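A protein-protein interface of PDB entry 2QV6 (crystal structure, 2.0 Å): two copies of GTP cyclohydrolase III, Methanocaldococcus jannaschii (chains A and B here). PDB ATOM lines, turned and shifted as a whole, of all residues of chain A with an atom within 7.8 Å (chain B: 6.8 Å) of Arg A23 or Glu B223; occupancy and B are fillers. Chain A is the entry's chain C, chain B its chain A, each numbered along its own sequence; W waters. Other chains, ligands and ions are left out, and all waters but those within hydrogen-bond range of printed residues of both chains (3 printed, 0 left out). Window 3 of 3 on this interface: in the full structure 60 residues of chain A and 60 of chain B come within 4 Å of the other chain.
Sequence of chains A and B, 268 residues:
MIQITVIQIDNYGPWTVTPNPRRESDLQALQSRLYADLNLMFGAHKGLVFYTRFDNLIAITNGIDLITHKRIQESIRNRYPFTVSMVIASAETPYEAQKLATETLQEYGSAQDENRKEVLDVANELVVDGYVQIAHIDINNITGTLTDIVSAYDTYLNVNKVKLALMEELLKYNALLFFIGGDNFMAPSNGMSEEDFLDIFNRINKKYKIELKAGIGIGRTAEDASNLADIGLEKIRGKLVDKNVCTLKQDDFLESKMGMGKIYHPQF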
ATOM      1  N   THR A  16     -20.864 -17.441  20.829  1.00  0.00           N
ATOM      2  CA  THR A  16     -20.425 -16.257  21.585  1.00  0.00           C
ATOM      3  C   THR A  16     -19.011 -16.388  22.142  1.00  0.00           C
ATOM      4  O   THR A  16     -18.439 -15.390  22.585  1.00  0.00           O
ATOM      5  CB  THR A  16     -21.371 -15.928  22.789  1.00  0.00           C
ATOM      6  OG1 THR A  16     -21.284 -16.958  23.785  1.00  0.00           O
ATOM      7  CG2 THR A  16     -22.831 -15.801  22.372  1.00  0.00           C
ATOM      8  N   ASN A  20     -13.221 -17.239  20.140  1.00  0.00           N
ATOM      9  CA  ASN A  20     -13.009 -16.570  21.443  1.00  0.00           C
ATOM     10  C   ASN A  20     -14.248 -15.810  21.913  1.00  0.00           C
ATOM     11  O   ASN A  20     -15.176 -15.588  21.134  1.00  0.00           O
ATOM     12  CB  ASN A  20     -11.876 -15.545  21.387  1.00  0.00           C
ATOM     13  CG  ASN A  20     -10.965 -15.756  20.226  1.00  0.00           C
ATOM     14  OD1 ASN A  20     -10.205 -16.725  20.202  1.00  0.00           O
ATOM     15  ND2 ASN A  20     -11.034 -14.856  19.236  1.00  0.00           N
ATOM     16  N   PRO A  21     -14.239 -15.372  23.184  1.00  0.00           N
ATOM     17  CA  PRO A  21     -15.289 -14.453  23.670  1.00  0.00           C
ATOM     18  C   PRO A  21     -15.304 -13.113  22.916  1.00  0.00           C
ATOM     19  O   PRO A  21     -14.276 -12.684  22.386  1.00  0.00           O
ATOM     20  CB  PRO A  21     -14.919 -14.225  25.148  1.00  0.00           C
ATOM     21  CG  PRO A  21     -13.976 -15.379  25.504  1.00  0.00           C
ATOM     22  CD  PRO A  21     -13.250 -15.699  24.237  1.00  0.00           C
ATOM     23  N   ARG A  22     -16.470 -12.471  22.894  1.00  0.00           N
ATOM     24  CA  ARG A  22     -16.710 -11.273  22.100  1.00  0.00           C
ATOM     25  C   ARG A  22     -17.033 -10.089  22.989  1.00  0.00           C
ATOM     26  O   ARG A  22     -17.743 -10.245  23.955  1.00  0.00           O
ATOM     27  CB  ARG A  22     -17.882 -11.536  21.199  1.00  0.00           C
ATOM     28  CG  ARG A  22     -17.696 -12.749  20.311  1.00  0.00           C
ATOM     29  CD  ARG A  22     -18.873 -12.990  19.437  1.00  0.00           C
ATOM     30  NE  ARG A  22     -18.763 -14.277  18.761  1.00  0.00           N
ATOM     31  CZ  ARG A  22     -18.158 -14.492  17.588  1.00  0.00           C
ATOM     32  NH1 ARG A  22     -17.619 -13.515  16.893  1.00  0.00           N
ATOM     33  NH2 ARG A  22     -18.128 -15.716  17.077  1.00  0.00           N
ATOM     34  N   ARG A  23     -16.531  -8.903  22.648  1.00  0.00           N
ATOM     35  CA  ARG A  23     -16.861  -7.667  23.367  1.00  0.00           C
ATOM     36  C   ARG A  23     -18.357  -7.600  23.668  1.00  0.00           C
ATOM     37  O   ARG A  23     -19.175  -7.729  22.746  1.00  0.00           O
ATOM     38  CB  ARG A  23     -16.519  -6.446  22.531  1.00  0.00           C
ATOM     39  CG  ARG A  23     -15.047  -6.159  22.473  1.00  0.00           C
ATOM     40  CD  ARG A  23     -14.684  -5.116  21.398  1.00  0.00           C
ATOM     41  NE  ARG A  23     -15.326  -3.836  21.649  1.00  0.00           N
ATOM     42  CZ  ARG A  23     -15.978  -3.123  20.740  1.00  0.00           C
ATOM     43  NH1 ARG A  23     -16.093  -3.559  19.484  1.00  0.00           N
ATOM     44  NH2 ARG A  23     -16.532  -1.960  21.093  1.00  0.00           N
ATOM     45  N   GLU A  24     -18.699  -7.367  24.934  1.00  0.00           N
ATOM     46  CA  GLU A  24     -20.093  -7.374  25.377  1.00  0.00           C
ATOM     47  C   GLU A  24     -20.953  -6.257  24.772  1.00  0.00           C
ATOM     48  O   GLU A  24     -22.114  -6.510  24.441  1.00  0.00           O
ATOM     49  CB  GLU A  24     -20.169  -7.327  26.911  1.00  0.00           C
ATOM     50  CG  GLU A  24     -21.555  -7.609  27.491  1.00  0.00           C
ATOM     51  CD  GLU A  24     -22.158  -8.942  27.040  1.00  0.00           C
ATOM     52  OE1 GLU A  24     -21.452  -9.977  26.994  1.00  0.00           O
ATOM     53  OE2 GLU A  24     -23.363  -8.958  26.748  1.00  0.00           O
ATOM     54  N   SER A  25     -20.385  -5.054  24.618  1.00  0.00           N
ATOM     55  CA  SER A  25     -21.041  -3.922  23.936  1.00  0.00           C
ATOM     56  C   SER A  25     -21.511  -4.299  22.537  1.00  0.00           C
ATOM     57  O   SER A  25     -22.625  -3.924  22.139  1.00  0.00           O
ATOM     58  CB  SER A  25     -20.115  -2.695  23.841  1.00  0.00           C
ATOM     59  OG  SER A  25     -18.981  -2.979  23.066  1.00  0.00           O
ATOM     60  N   ASP A  26     -20.705  -5.079  21.811  1.00  0.00           N
ATOM     61  CA  ASP A  26     -21.170  -5.689  20.511  1.00  0.00           C
ATOM     62  C   ASP A  26     -22.346  -6.663  20.627  1.00  0.00           C
ATOM     63  O   ASP A  26     -23.246  -6.669  19.771  1.00  0.00           O
ATOM     64  CB  ASP A  26     -20.035  -6.385  19.769  1.00  0.00           C
ATOM     65  CG  ASP A  26     -19.108  -5.442  19.108  1.00  0.00           C
ATOM     66  OD1 ASP A  26     -19.536  -4.336  18.723  1.00  0.00           O
ATOM     67  OD2 ASP A  26     -17.920  -5.792  18.988  1.00  0.00           O
ATOM     68  N   LEU A  27     -22.310  -7.508  21.649  1.00  0.00           N
ATOM     69  CA  LEU A  27     -23.349  -8.512  21.866  1.00  0.00           C
ATOM     70  C   LEU A  27     -24.665  -7.868  22.251  1.00  0.00           C
ATOM     71  O   LEU A  27     -25.734  -8.346  21.853  1.00  0.00           O
ATOM     72  CB  LEU A  27     -22.927  -9.552  22.928  1.00  0.00           C
ATOM     73  CG  LEU A  27     -21.856 -10.586  22.512  1.00  0.00           C
ATOM     74  CD1 LEU A  27     -21.671 -11.593  23.614  1.00  0.00           C
ATOM     75  CD2 LEU A  27     -22.178 -11.324  21.211  1.00  0.00           C
ATOM     76  N   GLN A  28     -24.594  -6.757  22.986  1.00  0.00           N
ATOM     77  CA  GLN A  28     -25.791  -5.991  23.338  1.00  0.00           C
ATOM     78  C   GLN A  28     -26.450  -5.318  22.142  1.00  0.00           C
ATOM     79  O   GLN A  28     -27.687  -5.394  21.982  1.00  0.00           O
ATOM     80  CB  GLN A  28     -25.496  -4.986  24.448  1.00  0.00           C
ATOM     81  CG  GLN A  28     -25.112  -5.647  25.726  1.00  0.00           C
ATOM     82  CD  GLN A  28     -26.177  -6.593  26.256  1.00  0.00           C
ATOM     83  OE1 GLN A  28     -25.922  -7.790  26.456  1.00  0.00           O
ATOM     84  NE2 GLN A  28     -27.341  -6.067  26.518  1.00  0.00           N
ATOM     85  N   ALA A  29     -25.629  -4.718  21.283  1.00  0.00           N
ATOM     86  CA  ALA A  29     -26.091  -4.109  20.015  1.00  0.00           C
ATOM     87  C   ALA A  29     -26.678  -5.180  19.064  1.00  0.00           C
ATOM     88  O   ALA A  29     -27.789  -5.009  18.529  1.00  0.00           O
ATOM     89  CB  ALA A  29     -24.936  -3.297  19.327  1.00  0.00           C
ATOM     90  N   ASN B  39     -24.612   1.627  22.968  1.00  0.00           N
ATOM     91  CA  ASN B  39     -23.504   0.668  23.101  1.00  0.00           C
ATOM     92  C   ASN B  39     -22.478   0.709  21.966  1.00  0.00           C
ATOM     93  O   ASN B  39     -21.307   0.505  22.216  1.00  0.00           O
ATOM     94  CB  ASN B  39     -23.991  -0.790  23.287  1.00  0.00           C
ATOM     95  CG  ASN B  39     -24.067  -1.207  24.734  1.00  0.00           C
ATOM     96  OD1 ASN B  39     -25.096  -1.666  25.195  1.00  0.00           O
ATOM     97  ND2 ASN B  39     -22.989  -0.971  25.492  1.00  0.00           N
ATOM     98  N   LEU B  40     -22.900   0.945  20.720  1.00  0.00           N
ATOM     99  CA  LEU B  40     -21.904   1.109  19.657  1.00  0.00           C
ATOM    100  C   LEU B  40     -21.044   2.368  19.868  1.00  0.00           C
ATOM    101  O   LEU B  40     -19.814   2.283  19.748  1.00  0.00           O
ATOM    102  CB  LEU B  40     -22.528   1.142  18.262  1.00  0.00           C
ATOM    103  CG  LEU B  40     -23.166  -0.145  17.729  1.00  0.00           C
ATOM    104  CD1 LEU B  40     -23.577   0.101  16.307  1.00  0.00           C
ATOM    105  CD2 LEU B  40     -22.208  -1.328  17.833  1.00  0.00           C
ATOM    106  N   PHE B  42     -20.749   4.631  22.690  1.00  0.00           N
ATOM    107  CA  PHE B  42     -19.947   4.509  23.934  1.00  0.00           C
ATOM    108  C   PHE B  42     -18.949   3.365  23.850  1.00  0.00           C
ATOM    109  O   PHE B  42     -17.876   3.475  24.392  1.00  0.00           O
ATOM    110  CB  PHE B  42     -20.816   4.318  25.173  1.00  0.00           C
ATOM    111  CG  PHE B  42     -21.417   5.589  25.689  1.00  0.00           C
ATOM    112  CD1 PHE B  42     -20.630   6.519  26.380  1.00  0.00           C
ATOM    113  CD2 PHE B  42     -22.771   5.848  25.556  1.00  0.00           C
ATOM    114  CE1 PHE B  42     -21.175   7.704  26.862  1.00  0.00           C
ATOM    115  CE2 PHE B  42     -23.325   7.032  26.049  1.00  0.00           C
ATOM    116  CZ  PHE B  42     -22.509   7.964  26.711  1.00  0.00           C
ATOM    117  N   GLY B  43     -19.324   2.274  23.176  1.00  0.00           N
ATOM    118  CA  GLY B  43     -18.434   1.159  22.930  1.00  0.00           C
ATOM    119  C   GLY B  43     -17.243   1.555  22.105  1.00  0.00           C
ATOM    120  O   GLY B  43     -16.167   1.035  22.314  1.00  0.00           O
ATOM    121  N   ALA B  44     -17.446   2.483  21.171  1.00  0.00           N
ATOM    122  CA  ALA B  44     -16.362   3.054  20.377  1.00  0.00           C
ATOM    123  C   ALA B  44     -15.291   3.654  21.228  1.00  0.00           C
ATOM    124  O   ALA B  44     -14.173   3.747  20.764  1.00  0.00           O
ATOM    125  CB  ALA B  44     -16.874   4.126  19.390  1.00  0.00           C
ATOM    126  N   HIS B  45     -15.623   4.110  22.433  1.00  0.00           N
ATOM    127  CA  HIS B  45     -14.621   4.702  23.333  1.00  0.00           C
ATOM    128  C   HIS B  45     -14.421   3.862  24.572  1.00  0.00           C
ATOM    129  O   HIS B  45     -14.075   4.402  25.611  1.00  0.00           O
ATOM    130  CB  HIS B  45     -15.029   6.131  23.730  1.00  0.00           C
ATOM    131  CG  HIS B  45     -15.150   7.069  22.572  1.00  0.00           C
ATOM    132  ND1 HIS B  45     -14.099   7.836  22.124  1.00  0.00           N
ATOM    133  CD2 HIS B  45     -16.200   7.361  21.764  1.00  0.00           C
ATOM    134  CE1 HIS B  45     -14.493   8.560  21.092  1.00  0.00           C
ATOM    135  NE2 HIS B  45     -15.762   8.287  20.848  1.00  0.00           N
ATOM    136  N   LYS B  46     -14.656   2.554  24.452  1.00  0.00           N
ATOM    137  CA  LYS B  46     -14.447   1.568  25.517  1.00  0.00           C
ATOM    138  C   LYS B  46     -15.406   1.641  26.731  1.00  0.00           C
ATOM    139  O   LYS B  46     -15.065   1.183  27.825  1.00  0.00           O
ATOM    140  CB  LYS B  46     -12.994   1.569  26.004  1.00  0.00           C
ATOM    141  CG  LYS B  46     -11.950   1.484  24.895  1.00  0.00           C
ATOM    142  CD  LYS B  46     -10.924   0.420  25.228  1.00  0.00           C
ATOM    143  CE  LYS B  46      -9.485   0.908  25.125  1.00  0.00           C
ATOM    144  NZ  LYS B  46      -8.585  -0.173  25.661  1.00  0.00           N
ATOM    145  N   GLY B  47     -16.598   2.194  26.530  1.00  0.00           N
ATOM    146  CA  GLY B  47     -17.659   2.101  27.516  1.00  0.00           C
ATOM    147  C   GLY B  47     -18.612   0.921  27.346  1.00  0.00           C
ATOM    148  O   GLY B  47     -18.497   0.106  26.415  1.00  0.00           O
ATOM    149  N   LEU B  48     -19.564   0.836  28.270  1.00  0.00           N
ATOM    150  CA  LEU B  48     -20.590  -0.203  28.242  1.00  0.00           C
ATOM    151  C   LEU B  48     -21.834   0.371  28.900  1.00  0.00           C
ATOM    152  O   LEU B  48     -21.730   1.026  29.939  1.00  0.00           O
ATOM    153  CB  LEU B  48     -20.103  -1.446  28.993  1.00  0.00           C
ATOM    154  CG  LEU B  48     -20.984  -2.686  29.017  1.00  0.00           C
ATOM    155  CD1 LEU B  48     -21.270  -3.200  27.615  1.00  0.00           C
ATOM    156  CD2 LEU B  48     -20.294  -3.748  29.858  1.00  0.00           C
ATOM    157  N   ILE B  60     -21.065   2.695  32.252  1.00  0.00           N
ATOM    158  CA  ILE B  60     -19.755   2.864  32.910  1.00  0.00           C
ATOM    159  C   ILE B  60     -18.892   3.554  31.886  1.00  0.00           C
ATOM    160  O   ILE B  60     -18.737   3.044  30.779  1.00  0.00           O
ATOM    161  CB  ILE B  60     -19.128   1.520  33.332  1.00  0.00           C
ATOM    162  CG1 ILE B  60     -20.059   0.777  34.269  1.00  0.00           C
ATOM    163  CG2 ILE B  60     -17.820   1.740  34.054  1.00  0.00           C
ATOM    164  CD1 ILE B  60     -19.674  -0.686  34.447  1.00  0.00           C
ATOM    165  N   VAL B 132     -12.462   0.025  37.020  1.00  0.00           N
ATOM    166  CA  VAL B 132     -13.743  -0.661  37.123  1.00  0.00           C
ATOM    167  C   VAL B 132     -13.508  -2.162  37.401  1.00  0.00           C
ATOM    168  O   VAL B 132     -12.571  -2.761  36.891  1.00  0.00           O
ATOM    169  CB  VAL B 132     -14.727  -0.346  35.904  1.00  0.00           C
ATOM    170  CG1 VAL B 132     -14.079   0.512  34.850  1.00  0.00           C
ATOM    171  CG2 VAL B 132     -15.269  -1.584  35.313  1.00  0.00           C
ATOM    172  N   ILE B 134     -15.738  -5.646  37.195  1.00  0.00           N
ATOM    173  CA  ILE B 134     -16.986  -6.223  36.704  1.00  0.00           C
ATOM    174  C   ILE B 134     -16.953  -7.705  36.955  1.00  0.00           C
ATOM    175  O   ILE B 134     -15.962  -8.340  36.624  1.00  0.00           O
ATOM    176  CB  ILE B 134     -17.198  -5.962  35.159  1.00  0.00           C
ATOM    177  CG1 ILE B 134     -17.484  -4.481  34.897  1.00  0.00           C
ATOM    178  CG2 ILE B 134     -18.326  -6.784  34.629  1.00  0.00           C
ATOM    179  CD1 ILE B 134     -18.051  -4.203  33.521  1.00  0.00           C
ATOM    180  N   ARG B 220      -8.784  -0.662  33.600  1.00  0.00           N
ATOM    181  CA  ARG B 220      -8.918   0.782  33.518  1.00  0.00           C
ATOM    182  C   ARG B 220     -10.260   1.283  32.932  1.00  0.00           C
ATOM    183  O   ARG B 220     -10.722   2.386  33.288  1.00  0.00           O
ATOM    184  CB  ARG B 220      -7.748   1.375  32.721  1.00  0.00           C
ATOM    185  CG  ARG B 220      -7.944   2.875  32.428  1.00  0.00           C
ATOM    186  CD  ARG B 220      -6.707   3.597  31.839  1.00  0.00           C
ATOM    187  NE  ARG B 220      -6.988   5.039  31.690  1.00  0.00           N
ATOM    188  CZ  ARG B 220      -6.264   6.041  32.212  1.00  0.00           C
ATOM    189  NH1 ARG B 220      -5.145   5.817  32.924  1.00  0.00           N
ATOM    190  NH2 ARG B 220      -6.659   7.303  32.011  1.00  0.00           N
ATOM    191  N   THR B 221     -10.865   0.494  32.039  1.00  0.00           N
ATOM    192  CA  THR B 221     -12.126   0.857  31.371  1.00  0.00           C
ATOM    193  C   THR B 221     -13.143  -0.291  31.515  1.00  0.00           C
ATOM    194  O   THR B 221     -12.775  -1.423  31.810  1.00  0.00           O
ATOM    195  CB  THR B 221     -11.925   1.207  29.846  1.00  0.00           C
ATOM    196  OG1 THR B 221     -11.483   0.065  29.116  1.00  0.00           O
ATOM    197  CG2 THR B 221     -10.903   2.335  29.645  1.00  0.00           C
ATOM    198  N   ALA B 222     -14.426   0.018  31.338  1.00  0.00           N
ATOM    199  CA  ALA B 222     -15.469  -1.022  31.267  1.00  0.00           C
ATOM    200  C   ALA B 222     -15.104  -2.139  30.282  1.00  0.00           C
ATOM    201  O   ALA B 222     -15.217  -3.304  30.617  1.00  0.00           O
ATOM    202  CB  ALA B 222     -16.818  -0.409  30.915  1.00  0.00           C
ATOM    203  N   GLU B 223     -14.629  -1.786  29.087  1.00  0.00           N
ATOM    204  CA  GLU B 223     -14.241  -2.777  28.059  1.00  0.00           C
ATOM    205  C   GLU B 223     -13.172  -3.756  28.539  1.00  0.00           C
ATOM    206  O   GLU B 223     -13.296  -4.954  28.355  1.00  0.00           O
ATOM    207  CB  GLU B 223     -13.739  -2.090  26.790  1.00  0.00           C
ATOM    208  CG  GLU B 223     -13.545  -3.055  25.652  1.00  0.00           C
ATOM    209  CD  GLU B 223     -13.616  -2.407  24.280  1.00  0.00           C
ATOM    210  OE1 GLU B 223     -14.674  -1.839  23.909  1.00  0.00           O
ATOM    211  OE2 GLU B 223     -12.611  -2.486  23.550  1.00  0.00           O
ATOM    212  N   ASP B 224     -12.117  -3.225  29.160  1.00  0.00           N
ATOM    213  CA  ASP B 224     -11.008  -4.032  29.664  1.00  0.00           C
ATOM    214  C   ASP B 224     -11.498  -4.957  30.763  1.00  0.00           C
ATOM    215  O   ASP B 224     -11.178  -6.150  30.764  1.00  0.00           O
ATOM    216  CB  ASP B 224      -9.899  -3.116  30.230  1.00  0.00           C
ATOM    217  CG  ASP B 224      -9.289  -2.207  29.173  1.00  0.00           C
ATOM    218  OD1 ASP B 224      -8.910  -2.733  28.115  1.00  0.00           O
ATOM    219  OD2 ASP B 224      -9.182  -0.976  29.384  1.00  0.00           O
ATOM    220  N   ALA B 225     -12.272  -4.386  31.693  1.00  0.00           N
ATOM    221  CA  ALA B 225     -12.843  -5.135  32.831  1.00  0.00           C
ATOM    222  C   ALA B 225     -13.686  -6.313  32.372  1.00  0.00           C
ATOM    223  O   ALA B 225     -13.537  -7.409  32.902  1.00  0.00           O
ATOM    224  CB  ALA B 225     -13.683  -4.212  33.730  1.00  0.00           C
ATOM    225  N   SER B 226     -14.569  -6.089  31.389  1.00  0.00           N
ATOM    226  CA  SER B 226     -15.528  -7.121  30.983  1.00  0.00           C
ATOM    227  C   SER B 226     -14.894  -8.188  30.098  1.00  0.00           C
ATOM    228  O   SER B 226     -15.353  -9.324  30.054  1.00  0.00           O
ATOM    229  CB  SER B 226     -16.733  -6.493  30.272  1.00  0.00           C
ATOM    230  OG  SER B 226     -16.331  -5.887  29.059  1.00  0.00           O
ATOM    231  N   ASN B 227     -13.856  -7.800  29.362  1.00  0.00           N
ATOM    232  CA  ASN B 227     -13.075  -8.742  28.579  1.00  0.00           C
ATOM    233  C   ASN B 227     -12.321  -9.715  29.480  1.00  0.00           C
ATOM    234  O   ASN B 227     -12.291 -10.910  29.207  1.00  0.00           O
ATOM    235  CB  ASN B 227     -12.097  -8.002  27.655  1.00  0.00           C
ATOM    236  CG  ASN B 227     -12.750  -7.475  26.367  1.00  0.00           C
ATOM    237  OD1 ASN B 227     -13.940  -7.692  26.084  1.00  0.00           O
ATOM    238  ND2 ASN B 227     -11.949  -6.766  25.579  1.00  0.00           N
ATOM    239  N   LEU B 228     -11.693  -9.190  30.531  1.00  0.00           N
ATOM    240  CA  LEU B 228     -11.020 -10.015  31.539  1.00  0.00           C
ATOM    241  C   LEU B 228     -12.014 -10.917  32.298  1.00  0.00           C
ATOM    242  O   LEU B 228     -11.714 -12.067  32.606  1.00  0.00           O
ATOM    243  CB  LEU B 228     -10.235  -9.126  32.526  1.00  0.00           C
ATOM    244  CG  LEU B 228      -8.991  -8.456  31.927  1.00  0.00           C
ATOM    245  CD1 LEU B 228      -8.417  -7.360  32.876  1.00  0.00           C
ATOM    246  CD2 LEU B 228      -7.936  -9.495  31.578  1.00  0.00           C
ATOM    247  N   ASP B 230     -14.678 -12.171  30.986  1.00  0.00           N
ATOM    248  CA  ASP B 230     -15.028 -13.248  30.039  1.00  0.00           C
ATOM    249  C   ASP B 230     -13.988 -14.374  30.018  1.00  0.00           C
ATOM    250  O   ASP B 230     -14.323 -15.557  29.949  1.00  0.00           O
ATOM    251  CB  ASP B 230     -15.163 -12.707  28.605  1.00  0.00           C
ATOM    252  CG  ASP B 230     -16.480 -11.987  28.348  1.00  0.00           C
ATOM    253  OD1 ASP B 230     -17.504 -12.265  29.000  1.00  0.00           O
ATOM    254  OD2 ASP B 230     -16.501 -11.124  27.447  1.00  0.00           O
HETATM  255  O   HOH W   1     -17.232  -1.883  24.696  1.00  0.00           O
HETATM  256  O   HOH W   2     -18.465   0.046  19.188  1.00  0.00           O
HETATM  257  O   HOH W   3     -16.754  -8.180  26.958  1.00  0.00           O
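N of Glu B223 lies within hydrogen-bond range of O of Lys B46 (3.3 Å).
The backbone NH of Ile B60 sits at hydrogen-bond distance from the backbone carbonyl oxygen of Leu B48 (2.9 Å).
O of Glu B223 sits at hydrogen-bond distance from OG of Ser B226 (3.3 Å).
The side-chain hydroxyl (OG) of Ser A25 sits at hydrogen-bond distance from the guanidinium group (NH2) of Arg A23, 3.3 Å away.
The guanidinium group of Arg A23 is in salt-bridge range of the side-chain carboxylate of Asp A26.
OE2 of Glu A24 lies close to OE1 of Gln A28, 2.8 Å away.
Of the printed residues of chain B, Arg A23 touches Gly B43, Glu B223 and Asn B227.
Of chain A, only Arg A23 comes within 4 Å of Glu B223.
No residue of chain A comes within 4 Å of Ala B222.
Printed residues of chain A within 4 Å of Asn B39: Ser A25 (3.6 Å) and Gln A28 (3.4 Å).
Printed residues of chain B within 4 Å of Arg A22: Asp B230 (3.8 Å).
The nearest residue of chain A that does not touch Glu B223 is Ser A25 (4.5 Å).
The nearest printed residue of chain B that does not touch Pro A21 is Asn B227 (5.9 Å).
The backbone carbonyl oxygen (O) of Gly B43 sits at hydrogen-bond distance from the guanidinium group (NH2) of Arg A23 (3.3 Å).
The side-chain carboxylate (OE1) of Glu B223 is in salt-bridge range of the guanidinium group (NE) of Arg A23 (3.1 Å).
Water W1 lies within hydrogen-bond range of the side-chain hydroxyl (OG) of Ser A25 (2.6 Å), the side-chain carboxylate (OE1) of Glu B223 (2.7 Å) and the backbone carbonyl oxygen (O) of Gly B47 (2.9 Å).
Water W2 lies within hydrogen-bond range of O of Leu B40 (2.7 Å), N of Ala B44 (3.3 Å) and NH2 of Arg A23 (3.4 Å).
Water W3 lies within hydrogen-bond range of the backbone NH (N) of Glu A24 (2.9 Å), the side-chain amide oxygen (OD1) of Asn B227 (3.0 Å), the side-chain carboxylate (OD2) of Asp B230 (3.0 Å) and the side-chain hydroxyl (OG) of Ser B226 (3.1 Å).
No position is printed for both chains.
Of the 9 pairs that touch across the chains among the printed residues, none has its exchanged pair printed and touching as well.
Printed residues of chain B that touch a printed residue of chain A: Asn B39, Leu B40, Gly B43, Leu B48, Glu B223, Asn B227 and Asp B230.
Hydrophobic or aromatic side chains of chain B within 4 Å of the printed part of chain A: Leu B40 and Leu B48.
Of the 11 printed residues of chain A, 6 touch a printed residue of chain B.
Hydrophobic or aromatic side chains of chain A that line the printed part of chain B: Pro A21 and Ala A29.
Along chain A the printed residues that touch a printed residue of chain B span positions 21 to 29.
Among the printed residues, Asp or Glu carboxylates within 4 Å of a Lys or Arg side-chain nitrogen of the other chain: Arg A23 with Glu B223.
Pro A21 touches Asp B230.
Arg A22 touches Asp B230 (O to OD2, 3.8 Å).
OD1 of Asn B227 touches CA of Arg A23, at 3.99 Å.
Ser A25 touches Asn B39 (O to CB, 3.6 Å).
Leu B48 touches Ser A25.
Asn B39 touches Gln A28 (OD1 to CB, 3.4 Å).
CB of Ala A29 touches CD2 of Leu B40 (3.7 Å).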
